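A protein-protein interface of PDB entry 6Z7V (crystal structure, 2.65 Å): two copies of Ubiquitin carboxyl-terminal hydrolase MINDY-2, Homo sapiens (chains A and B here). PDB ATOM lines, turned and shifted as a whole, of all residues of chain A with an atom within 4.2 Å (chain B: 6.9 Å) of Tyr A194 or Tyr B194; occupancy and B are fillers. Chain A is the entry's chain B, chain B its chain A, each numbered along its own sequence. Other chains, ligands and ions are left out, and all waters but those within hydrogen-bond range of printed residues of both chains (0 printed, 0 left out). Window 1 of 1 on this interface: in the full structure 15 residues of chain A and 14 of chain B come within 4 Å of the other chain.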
ATOM      1  N   ASP A 141     -30.333  -5.962  -8.142  1.00  0.00           N
ATOM      2  CA  ASP A 141     -29.114  -6.144  -8.908  1.00  0.00           C
ATOM      3  C   ASP A 141     -29.246  -7.435  -9.706  1.00  0.00           C
ATOM      4  O   ASP A 141     -29.284  -8.525  -9.118  1.00  0.00           O
ATOM      5  CB  ASP A 141     -27.918  -6.178  -7.960  1.00  0.00           C
ATOM      6  CG  ASP A 141     -26.594  -6.106  -8.676  1.00  0.00           C
ATOM      7  OD1 ASP A 141     -26.575  -6.086  -9.926  1.00  0.00           O
ATOM      8  OD2 ASP A 141     -25.563  -6.079  -7.969  1.00  0.00           O
ATOM      9  N   PRO A 142     -29.334  -7.359 -11.036  1.00  0.00           N
ATOM     10  CA  PRO A 142     -29.536  -8.583 -11.827  1.00  0.00           C
ATOM     11  C   PRO A 142     -28.367  -9.540 -11.774  1.00  0.00           C
ATOM     12  O   PRO A 142     -28.541 -10.720 -12.104  1.00  0.00           O
ATOM     13  CB  PRO A 142     -29.750  -8.050 -13.247  1.00  0.00           C
ATOM     14  CG  PRO A 142     -29.007  -6.773 -13.264  1.00  0.00           C
ATOM     15  CD  PRO A 142     -29.209  -6.172 -11.896  1.00  0.00           C
ATOM     16  N   THR A 193     -30.968   1.946  -5.368  1.00  0.00           N
ATOM     17  CA  THR A 193     -29.820   1.091  -5.625  1.00  0.00           C
ATOM     18  C   THR A 193     -29.053   1.626  -6.828  1.00  0.00           C
ATOM     19  O   THR A 193     -29.549   2.464  -7.586  1.00  0.00           O
ATOM     20  CB  THR A 193     -30.243  -0.362  -5.869  1.00  0.00           C
ATOM     21  OG1 THR A 193     -30.985  -0.446  -7.092  1.00  0.00           O
ATOM     22  CG2 THR A 193     -31.107  -0.867  -4.724  1.00  0.00           C
ATOM     23  N   TYR A 194     -27.827   1.124  -7.003  1.00  0.00           N
ATOM     24  CA  TYR A 194     -26.990   1.610  -8.092  1.00  0.00           C
ATOM     25  C   TYR A 194     -27.489   1.126  -9.446  1.00  0.00           C
ATOM     26  O   TYR A 194     -27.323   1.830 -10.449  1.00  0.00           O
ATOM     27  CB  TYR A 194     -25.533   1.213  -7.857  1.00  0.00           C
ATOM     28  CG  TYR A 194     -24.885   2.158  -6.872  1.00  0.00           C
ATOM     29  CD1 TYR A 194     -24.676   3.495  -7.197  1.00  0.00           C
ATOM     30  CD2 TYR A 194     -24.533   1.734  -5.600  1.00  0.00           C
ATOM     31  CE1 TYR A 194     -24.112   4.375  -6.290  1.00  0.00           C
ATOM     32  CE2 TYR A 194     -23.967   2.608  -4.685  1.00  0.00           C
ATOM     33  CZ  TYR A 194     -23.760   3.924  -5.034  1.00  0.00           C
ATOM     34  OH  TYR A 194     -23.196   4.786  -4.114  1.00  0.00           O
ATOM     35  N   HIS A 195     -28.119  -0.048  -9.500  1.00  0.00           N
ATOM     36  CA  HIS A 195     -28.806  -0.432 -10.726  1.00  0.00           C
ATOM     37  C   HIS A 195     -29.938   0.535 -11.029  1.00  0.00           C
ATOM     38  O   HIS A 195     -30.124   0.943 -12.181  1.00  0.00           O
ATOM     39  CB  HIS A 195     -29.349  -1.854 -10.621  1.00  0.00           C
ATOM     40  CG  HIS A 195     -30.041  -2.321 -11.862  1.00  0.00           C
ATOM     41  ND1 HIS A 195     -31.063  -3.245 -11.845  1.00  0.00           N
ATOM     42  CD2 HIS A 195     -29.851  -1.994 -13.163  1.00  0.00           C
ATOM     43  CE1 HIS A 195     -31.472  -3.469 -13.082  1.00  0.00           C
ATOM     44  NE2 HIS A 195     -30.752  -2.724 -13.900  1.00  0.00           N
ATOM     45  N   GLY A 196     -30.706   0.912 -10.005  1.00  0.00           N
ATOM     46  CA  GLY A 196     -31.767   1.880 -10.214  1.00  0.00           C
ATOM     47  C   GLY A 196     -31.236   3.219 -10.679  1.00  0.00           C
ATOM     48  O   GLY A 196     -31.779   3.826 -11.607  1.00  0.00           O
ATOM     49  N   LEU A 197     -30.156   3.689 -10.053  1.00  0.00           N
ATOM     50  CA  LEU A 197     -29.556   4.959 -10.449  1.00  0.00           C
ATOM     51  C   LEU A 197     -29.106   4.924 -11.907  1.00  0.00           C
ATOM     52  O   LEU A 197     -29.249   5.914 -12.633  1.00  0.00           O
ATOM     53  CB  LEU A 197     -28.388   5.284  -9.517  1.00  0.00           C
ATOM     54  CG  LEU A 197     -27.848   6.711  -9.561  1.00  0.00           C
ATOM     55  CD1 LEU A 197     -28.967   7.703  -9.328  1.00  0.00           C
ATOM     56  CD2 LEU A 197     -26.739   6.900  -8.543  1.00  0.00           C
ATOM     57  N   CYS A 198     -28.583   3.782 -12.356  1.00  0.00           N
ATOM     58  CA  CYS A 198     -28.216   3.629 -13.760  1.00  0.00           C
ATOM     59  C   CYS A 198     -29.436   3.729 -14.662  1.00  0.00           C
ATOM     60  O   CYS A 198     -29.456   4.509 -15.622  1.00  0.00           O
ATOM     61  CB  CYS A 198     -27.533   2.285 -13.971  1.00  0.00           C
ATOM     62  SG  CYS A 198     -25.773   2.387 -13.986  1.00  0.00           S
ATOM     63  N   ASN A 250     -25.276   9.268  -6.264  1.00  0.00           N
ATOM     64  CA  ASN A 250     -24.885   8.238  -5.310  1.00  0.00           C
ATOM     65  C   ASN A 250     -26.067   7.988  -4.384  1.00  0.00           C
ATOM     66  O   ASN A 250     -27.022   8.766  -4.350  1.00  0.00           O
ATOM     67  CB  ASN A 250     -23.637   8.643  -4.523  1.00  0.00           C
ATOM     68  CG  ASN A 250     -23.750  10.029  -3.922  1.00  0.00           C
ATOM     69  OD1 ASN A 250     -24.688  10.319  -3.181  1.00  0.00           O
ATOM     70  ND2 ASN A 250     -22.787  10.894  -4.234  1.00  0.00           N
ATOM     71  N   VAL A 251     -25.993   6.888  -3.623  1.00  0.00           N
ATOM     72  CA  VAL A 251     -27.099   6.528  -2.731  1.00  0.00           C
ATOM     73  C   VAL A 251     -26.948   7.091  -1.323  1.00  0.00           C
ATOM     74  O   VAL A 251     -27.884   6.963  -0.521  1.00  0.00           O
ATOM     75  CB  VAL A 251     -27.294   5.000  -2.627  1.00  0.00           C
ATOM     76  CG1 VAL A 251     -27.411   4.387  -4.006  1.00  0.00           C
ATOM     77  CG2 VAL A 251     -26.158   4.351  -1.836  1.00  0.00           C
ATOM     78  N   GLY B 137     -14.901  -0.509 -14.337  1.00  0.00           N
ATOM     79  CA  GLY B 137     -16.157  -0.396 -13.622  1.00  0.00           C
ATOM     80  C   GLY B 137     -16.439  -1.549 -12.684  1.00  0.00           C
ATOM     81  O   GLY B 137     -17.600  -1.791 -12.332  1.00  0.00           O
ATOM     82  N   LEU B 139     -16.733  -2.561  -9.525  1.00  0.00           N
ATOM     83  CA  LEU B 139     -16.885  -1.976  -8.203  1.00  0.00           C
ATOM     84  C   LEU B 139     -17.778  -2.836  -7.316  1.00  0.00           C
ATOM     85  O   LEU B 139     -18.724  -3.480  -7.779  1.00  0.00           O
ATOM     86  CB  LEU B 139     -17.457  -0.554  -8.291  1.00  0.00           C
ATOM     87  CG  LEU B 139     -16.655   0.537  -9.021  1.00  0.00           C
ATOM     88  CD1 LEU B 139     -17.034   1.910  -8.483  1.00  0.00           C
ATOM     89  CD2 LEU B 139     -15.150   0.327  -8.940  1.00  0.00           C
ATOM     90  N   VAL B 140     -17.467  -2.830  -6.028  1.00  0.00           N
ATOM     91  CA  VAL B 140     -18.280  -3.524  -5.039  1.00  0.00           C
ATOM     92  C   VAL B 140     -19.497  -2.672  -4.716  1.00  0.00           C
ATOM     93  O   VAL B 140     -19.408  -1.443  -4.633  1.00  0.00           O
ATOM     94  CB  VAL B 140     -17.443  -3.826  -3.782  1.00  0.00           C
ATOM     95  CG1 VAL B 140     -18.326  -4.003  -2.562  1.00  0.00           C
ATOM     96  CG2 VAL B 140     -16.596  -5.071  -4.006  1.00  0.00           C
ATOM     97  N   ASP B 141     -20.643  -3.313  -4.562  1.00  0.00           N
ATOM     98  CA  ASP B 141     -21.840  -2.609  -4.128  1.00  0.00           C
ATOM     99  C   ASP B 141     -21.710  -2.247  -2.653  1.00  0.00           C
ATOM    100  O   ASP B 141     -21.656  -3.153  -1.811  1.00  0.00           O
ATOM    101  CB  ASP B 141     -23.064  -3.488  -4.373  1.00  0.00           C
ATOM    102  CG  ASP B 141     -24.366  -2.739  -4.216  1.00  0.00           C
ATOM    103  OD1 ASP B 141     -24.329  -1.550  -3.836  1.00  0.00           O
ATOM    104  OD2 ASP B 141     -25.428  -3.352  -4.458  1.00  0.00           O
ATOM    105  N   PRO B 142     -21.643  -0.960  -2.290  1.00  0.00           N
ATOM    106  CA  PRO B 142     -21.447  -0.601  -0.875  1.00  0.00           C
ATOM    107  C   PRO B 142     -22.666  -0.820   0.003  1.00  0.00           C
ATOM    108  O   PRO B 142     -22.554  -0.663   1.227  1.00  0.00           O
ATOM    109  CB  PRO B 142     -21.086   0.887  -0.940  1.00  0.00           C
ATOM    110  CG  PRO B 142     -21.746   1.369  -2.182  1.00  0.00           C
ATOM    111  CD  PRO B 142     -21.656   0.229  -3.162  1.00  0.00           C
ATOM    112  N   GLN B 143     -23.822  -1.155  -0.563  1.00  0.00           N
ATOM    113  CA  GLN B 143     -24.985  -1.438   0.269  1.00  0.00           C
ATOM    114  C   GLN B 143     -24.975  -2.852   0.827  1.00  0.00           C
ATOM    115  O   GLN B 143     -25.771  -3.154   1.726  1.00  0.00           O
ATOM    116  CB  GLN B 143     -26.271  -1.198  -0.520  1.00  0.00           C
ATOM    117  CG  GLN B 143     -26.522   0.265  -0.808  1.00  0.00           C
ATOM    118  CD  GLN B 143     -27.777   0.495  -1.613  1.00  0.00           C
ATOM    119  OE1 GLN B 143     -28.016  -0.171  -2.619  1.00  0.00           O
ATOM    120  NE2 GLN B 143     -28.585   1.451  -1.182  1.00  0.00           N
ATOM    121  N   LEU B 192     -17.808  -5.667 -14.871  1.00  0.00           N
ATOM    122  CA  LEU B 192     -18.536  -4.407 -14.797  1.00  0.00           C
ATOM    123  C   LEU B 192     -19.765  -4.581 -13.916  1.00  0.00           C
ATOM    124  O   LEU B 192     -20.561  -5.504 -14.125  1.00  0.00           O
ATOM    125  CB  LEU B 192     -18.953  -3.917 -16.186  1.00  0.00           C
ATOM    126  CG  LEU B 192     -19.703  -2.584 -16.209  1.00  0.00           C
ATOM    127  CD1 LEU B 192     -18.787  -1.460 -15.757  1.00  0.00           C
ATOM    128  CD2 LEU B 192     -20.255  -2.300 -17.601  1.00  0.00           C
ATOM    129  N   THR B 193     -19.912  -3.696 -12.936  1.00  0.00           N
ATOM    130  CA  THR B 193     -21.071  -3.674 -12.057  1.00  0.00           C
ATOM    131  C   THR B 193     -21.823  -2.360 -12.230  1.00  0.00           C
ATOM    132  O   THR B 193     -21.291  -1.378 -12.757  1.00  0.00           O
ATOM    133  CB  THR B 193     -20.667  -3.851 -10.588  1.00  0.00           C
ATOM    134  OG1 THR B 193     -19.920  -2.707 -10.155  1.00  0.00           O
ATOM    135  CG2 THR B 193     -19.819  -5.096 -10.423  1.00  0.00           C
ATOM    136  N   TYR B 194     -23.074  -2.352 -11.771  1.00  0.00           N
ATOM    137  CA  TYR B 194     -23.894  -1.157 -11.919  1.00  0.00           C
ATOM    138  C   TYR B 194     -23.364  -0.003 -11.077  1.00  0.00           C
ATOM    139  O   TYR B 194     -23.524   1.161 -11.460  1.00  0.00           O
ATOM    140  CB  TYR B 194     -25.349  -1.478 -11.580  1.00  0.00           C
ATOM    141  CG  TYR B 194     -26.075  -2.055 -12.775  1.00  0.00           C
ATOM    142  CD1 TYR B 194     -26.378  -1.261 -13.872  1.00  0.00           C
ATOM    143  CD2 TYR B 194     -26.413  -3.400 -12.825  1.00  0.00           C
ATOM    144  CE1 TYR B 194     -27.022  -1.784 -14.979  1.00  0.00           C
ATOM    145  CE2 TYR B 194     -27.057  -3.932 -13.926  1.00  0.00           C
ATOM    146  CZ  TYR B 194     -27.359  -3.122 -15.001  1.00  0.00           C
ATOM    147  OH  TYR B 194     -28.002  -3.653 -16.099  1.00  0.00           O
ATOM    148  N   HIS B 195     -22.719  -0.296  -9.947  1.00  0.00           N
ATOM    149  CA  HIS B 195     -22.063   0.770  -9.196  1.00  0.00           C
ATOM    150  C   HIS B 195     -20.886   1.342  -9.981  1.00  0.00           C
ATOM    151  O   HIS B 195     -20.614   2.546  -9.914  1.00  0.00           O
ATOM    152  CB  HIS B 195     -21.607   0.252  -7.832  1.00  0.00           C
ATOM    153  CG  HIS B 195     -20.892   1.276  -7.008  1.00  0.00           C
ATOM    154  ND1 HIS B 195     -19.842   0.956  -6.175  1.00  0.00           N
ATOM    155  CD2 HIS B 195     -21.077   2.611  -6.884  1.00  0.00           C
ATOM    156  CE1 HIS B 195     -19.409   2.051  -5.577  1.00  0.00           C
ATOM    157  NE2 HIS B 195     -20.141   3.069  -5.989  1.00  0.00           N
ATOM    158  N   GLY B 196     -20.179   0.497 -10.732  1.00  0.00           N
ATOM    159  CA  GLY B 196     -19.126   1.001 -11.595  1.00  0.00           C
ATOM    160  C   GLY B 196     -19.654   1.907 -12.690  1.00  0.00           C
ATOM    161  O   GLY B 196     -19.067   2.954 -12.979  1.00  0.00           O
ATOM    162  N   LEU B 197     -20.772   1.523 -13.312  1.00  0.00           N
ATOM    163  CA  LEU B 197     -21.375   2.375 -14.331  1.00  0.00           C
ATOM    164  C   LEU B 197     -21.763   3.733 -13.760  1.00  0.00           C
ATOM    165  O   LEU B 197     -21.577   4.766 -14.415  1.00  0.00           O
ATOM    166  CB  LEU B 197     -22.595   1.688 -14.932  1.00  0.00           C
ATOM    167  CG  LEU B 197     -22.454   0.954 -16.259  1.00  0.00           C
ATOM    168  CD1 LEU B 197     -23.712   0.142 -16.508  1.00  0.00           C
ATOM    169  CD2 LEU B 197     -22.222   1.943 -17.379  1.00  0.00           C
ATOM    170  N   CYS B 198     -22.295   3.758 -12.536  1.00  0.00           N
ATOM    171  CA  CYS B 198     -22.684   5.031 -11.941  1.00  0.00           C
ATOM    172  C   CYS B 198     -21.470   5.889 -11.624  1.00  0.00           C
ATOM    173  O   CYS B 198     -21.496   7.109 -11.821  1.00  0.00           O
ATOM    174  CB  CYS B 198     -23.510   4.803 -10.678  1.00  0.00           C
ATOM    175  SG  CYS B 198     -25.246   4.487 -10.990  1.00  0.00           S
ATOM    176  N   GLU B 199     -20.399   5.278 -11.116  1.00  0.00           N
ATOM    177  CA  GLU B 199     -19.212   6.063 -10.812  1.00  0.00           C
ATOM    178  C   GLU B 199     -18.513   6.519 -12.089  1.00  0.00           C
ATOM    179  O   GLU B 199     -17.979   7.631 -12.142  1.00  0.00           O
ATOM    180  CB  GLU B 199     -18.255   5.269  -9.928  1.00  0.00           C
ATOM    181  CG  GLU B 199     -17.214   6.143  -9.245  1.00  0.00           C
ATOM    182  CD  GLU B 199     -16.529   5.452  -8.084  1.00  0.00           C
ATOM    183  OE1 GLU B 199     -17.172   5.272  -7.025  1.00  0.00           O
ATOM    184  OE2 GLU B 199     -15.339   5.093  -8.236  1.00  0.00           O
ATOM    185  N   HIS B 249     -24.687   1.687 -21.094  1.00  0.00           N
ATOM    186  CA  HIS B 249     -25.674   2.004 -20.071  1.00  0.00           C
ATOM    187  C   HIS B 249     -26.211   0.772 -19.355  1.00  0.00           C
ATOM    188  O   HIS B 249     -27.183   0.893 -18.597  1.00  0.00           O
ATOM    189  CB  HIS B 249     -26.831   2.813 -20.674  1.00  0.00           C
ATOM    190  CG  HIS B 249     -27.583   2.101 -21.757  1.00  0.00           C
ATOM    191  ND1 HIS B 249     -27.035   1.833 -22.993  1.00  0.00           N
ATOM    192  CD2 HIS B 249     -28.855   1.639 -21.802  1.00  0.00           C
ATOM    193  CE1 HIS B 249     -27.931   1.219 -23.746  1.00  0.00           C
ATOM    194  NE2 HIS B 249     -29.045   1.091 -23.048  1.00  0.00           N
ATOM    195  N   ASN B 250     -25.614  -0.399 -19.562  1.00  0.00           N
ATOM    196  CA  ASN B 250     -26.018  -1.606 -18.857  1.00  0.00           C
ATOM    197  C   ASN B 250     -24.860  -2.593 -18.867  1.00  0.00           C
ATOM    198  O   ASN B 250     -23.896  -2.442 -19.620  1.00  0.00           O
ATOM    199  CB  ASN B 250     -27.268  -2.239 -19.476  1.00  0.00           C
ATOM    200  CG  ASN B 250     -27.105  -2.531 -20.957  1.00  0.00           C
ATOM    201  OD1 ASN B 250     -26.328  -3.400 -21.349  1.00  0.00           O
ATOM    202  ND2 ASN B 250     -27.855  -1.811 -21.787  1.00  0.00           N
ATOM    203  N   VAL B 251     -24.970  -3.610 -18.006  1.00  0.00           N
ATOM    204  CA  VAL B 251     -23.980  -4.683 -17.951  1.00  0.00           C
ATOM    205  C   VAL B 251     -24.319  -5.840 -18.880  1.00  0.00           C
ATOM    206  O   VAL B 251     -23.567  -6.823 -18.927  1.00  0.00           O
ATOM    207  CB  VAL B 251     -23.825  -5.231 -16.516  1.00  0.00           C
ATOM    208  CG1 VAL B 251     -23.534  -4.109 -15.542  1.00  0.00           C
ATOM    209  CG2 VAL B 251     -25.081  -5.990 -16.106  1.00  0.00           C
ATOM    210  N   ASP B 252     -25.432  -5.763 -19.612  1.00  0.00           N
ATOM    211  CA  ASP B 252     -25.844  -6.834 -20.508  1.00  0.00           C
ATOM    212  C   ASP B 252     -25.121  -6.793 -21.847  1.00  0.00           C
ATOM    213  O   ASP B 252     -25.280  -7.722 -22.648  1.00  0.00           O
ATOM    214  CB  ASP B 252     -27.352  -6.760 -20.757  1.00  0.00           C
ATOM    215  CG  ASP B 252     -28.133  -6.424 -19.505  1.00  0.00           C
ATOM    216  OD1 ASP B 252     -27.834  -7.003 -18.439  1.00  0.00           O
ATOM    217  OD2 ASP B 252     -29.042  -5.570 -19.584  1.00  0.00           O
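Among the printed residues, pairs that only touch across the chains: His A195 with Tyr B194, Cys A198 with Leu B197, Pro A142 with Tyr B194, Tyr A194 with His B195, Leu A197 with Cys B198, Tyr A194 with Pro B142, Thr A193 with Gln B143, Tyr A194 with Asp B141, Val A251 with Gln B143, Asp A141 with Tyr B194 and Tyr A194 with Tyr B194.
Printed residues of chain A that touch a printed residue of chain B: Asp A141, Pro A142, Thr A193, Tyr A194, His A195, Leu A197, Cys A198 and Val A251. Hydrophobic or aromatic side chains of chain A that line the printed part of chain B: Pro A142, Tyr A194, His A195, Leu A197 and Val A251. Hydrophobic or aromatic side chains of chain B within 4 Å of the printed part of chain A: Pro B142, Tyr B194, His B195 and Leu B197. Among the printed residues, 14 pairs touch across the chains.
A ring nitrogen (ND1) of His B195 is in hydrogen-bond range of the backbone carbonyl oxygen (O) of Val B140 (2.9 Å). The side-chain carboxylate (OD1) of Asp B141 lies close to the backbone NH (N) of Gln B143 (3.3 Å). The backbone carbonyl oxygen of Tyr B194 lies close to the side-chain sulfur of Cys B198. N of Gly A196 lies within hydrogen-bond range of OG1 of Thr A193, at 3.2 Å.
Asp A141 touches Tyr B194, and with the chains exchanged Tyr A194 touches Asp B141. Tyr A194 touches its own counterpart, Tyr B194. Tyr A194 touches His B195, and with the chains exchanged His A195 touches Tyr B194. Cys A198 touches its own counterpart, Cys B198. Positions printed for both chains: 141, 142, 193, 194, 195, 196, 197, 198, 250 and 251. Of the 14 pairs that touch across the chains among the printed residues, 12 have their exchanged pair printed and touching as well.
SG of Cys A198 lies within hydrogen-bond range of O of Tyr B194 (3.6 Å). SG of Cys B198 is in hydrogen-bond range of O of Tyr A194, at 3.4 Å. SG of Cys B198 sits at hydrogen-bond distance from N of Cys A198.
Of the printed residues of chain B, Tyr A194 touches Asp B141 (3.7 Å), Pro B142 (3.6 Å), Tyr B194 (3.99 Å), His B195 (3.5 Å) and Cys B198 (3.4 Å). Of the printed residues of chain A, Tyr B194 touches Asp A141, Pro A142, Tyr A194, His A195 and Cys A198. Printed residues of chain B within 4 Å of Pro A142: Tyr B194 (3.5 Å). Of the printed residues of chain A, Gln B143 touches Thr A193 and Val A251. Of the printed residues of chain A, Leu B197 touches Cys A198 (3.4 Å). Of the printed residues of chain B, Asp A141 touches Tyr B194 (3.96 Å). Thr B193 touches none of the printed residues of chain A. The nearest printed residue of chain A that does not touch Tyr B194 is Gly A196 (6.1 Å). The nearest printed residue of chain B that does not touch Asp A141 is Asp B141 (4.4 Å).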
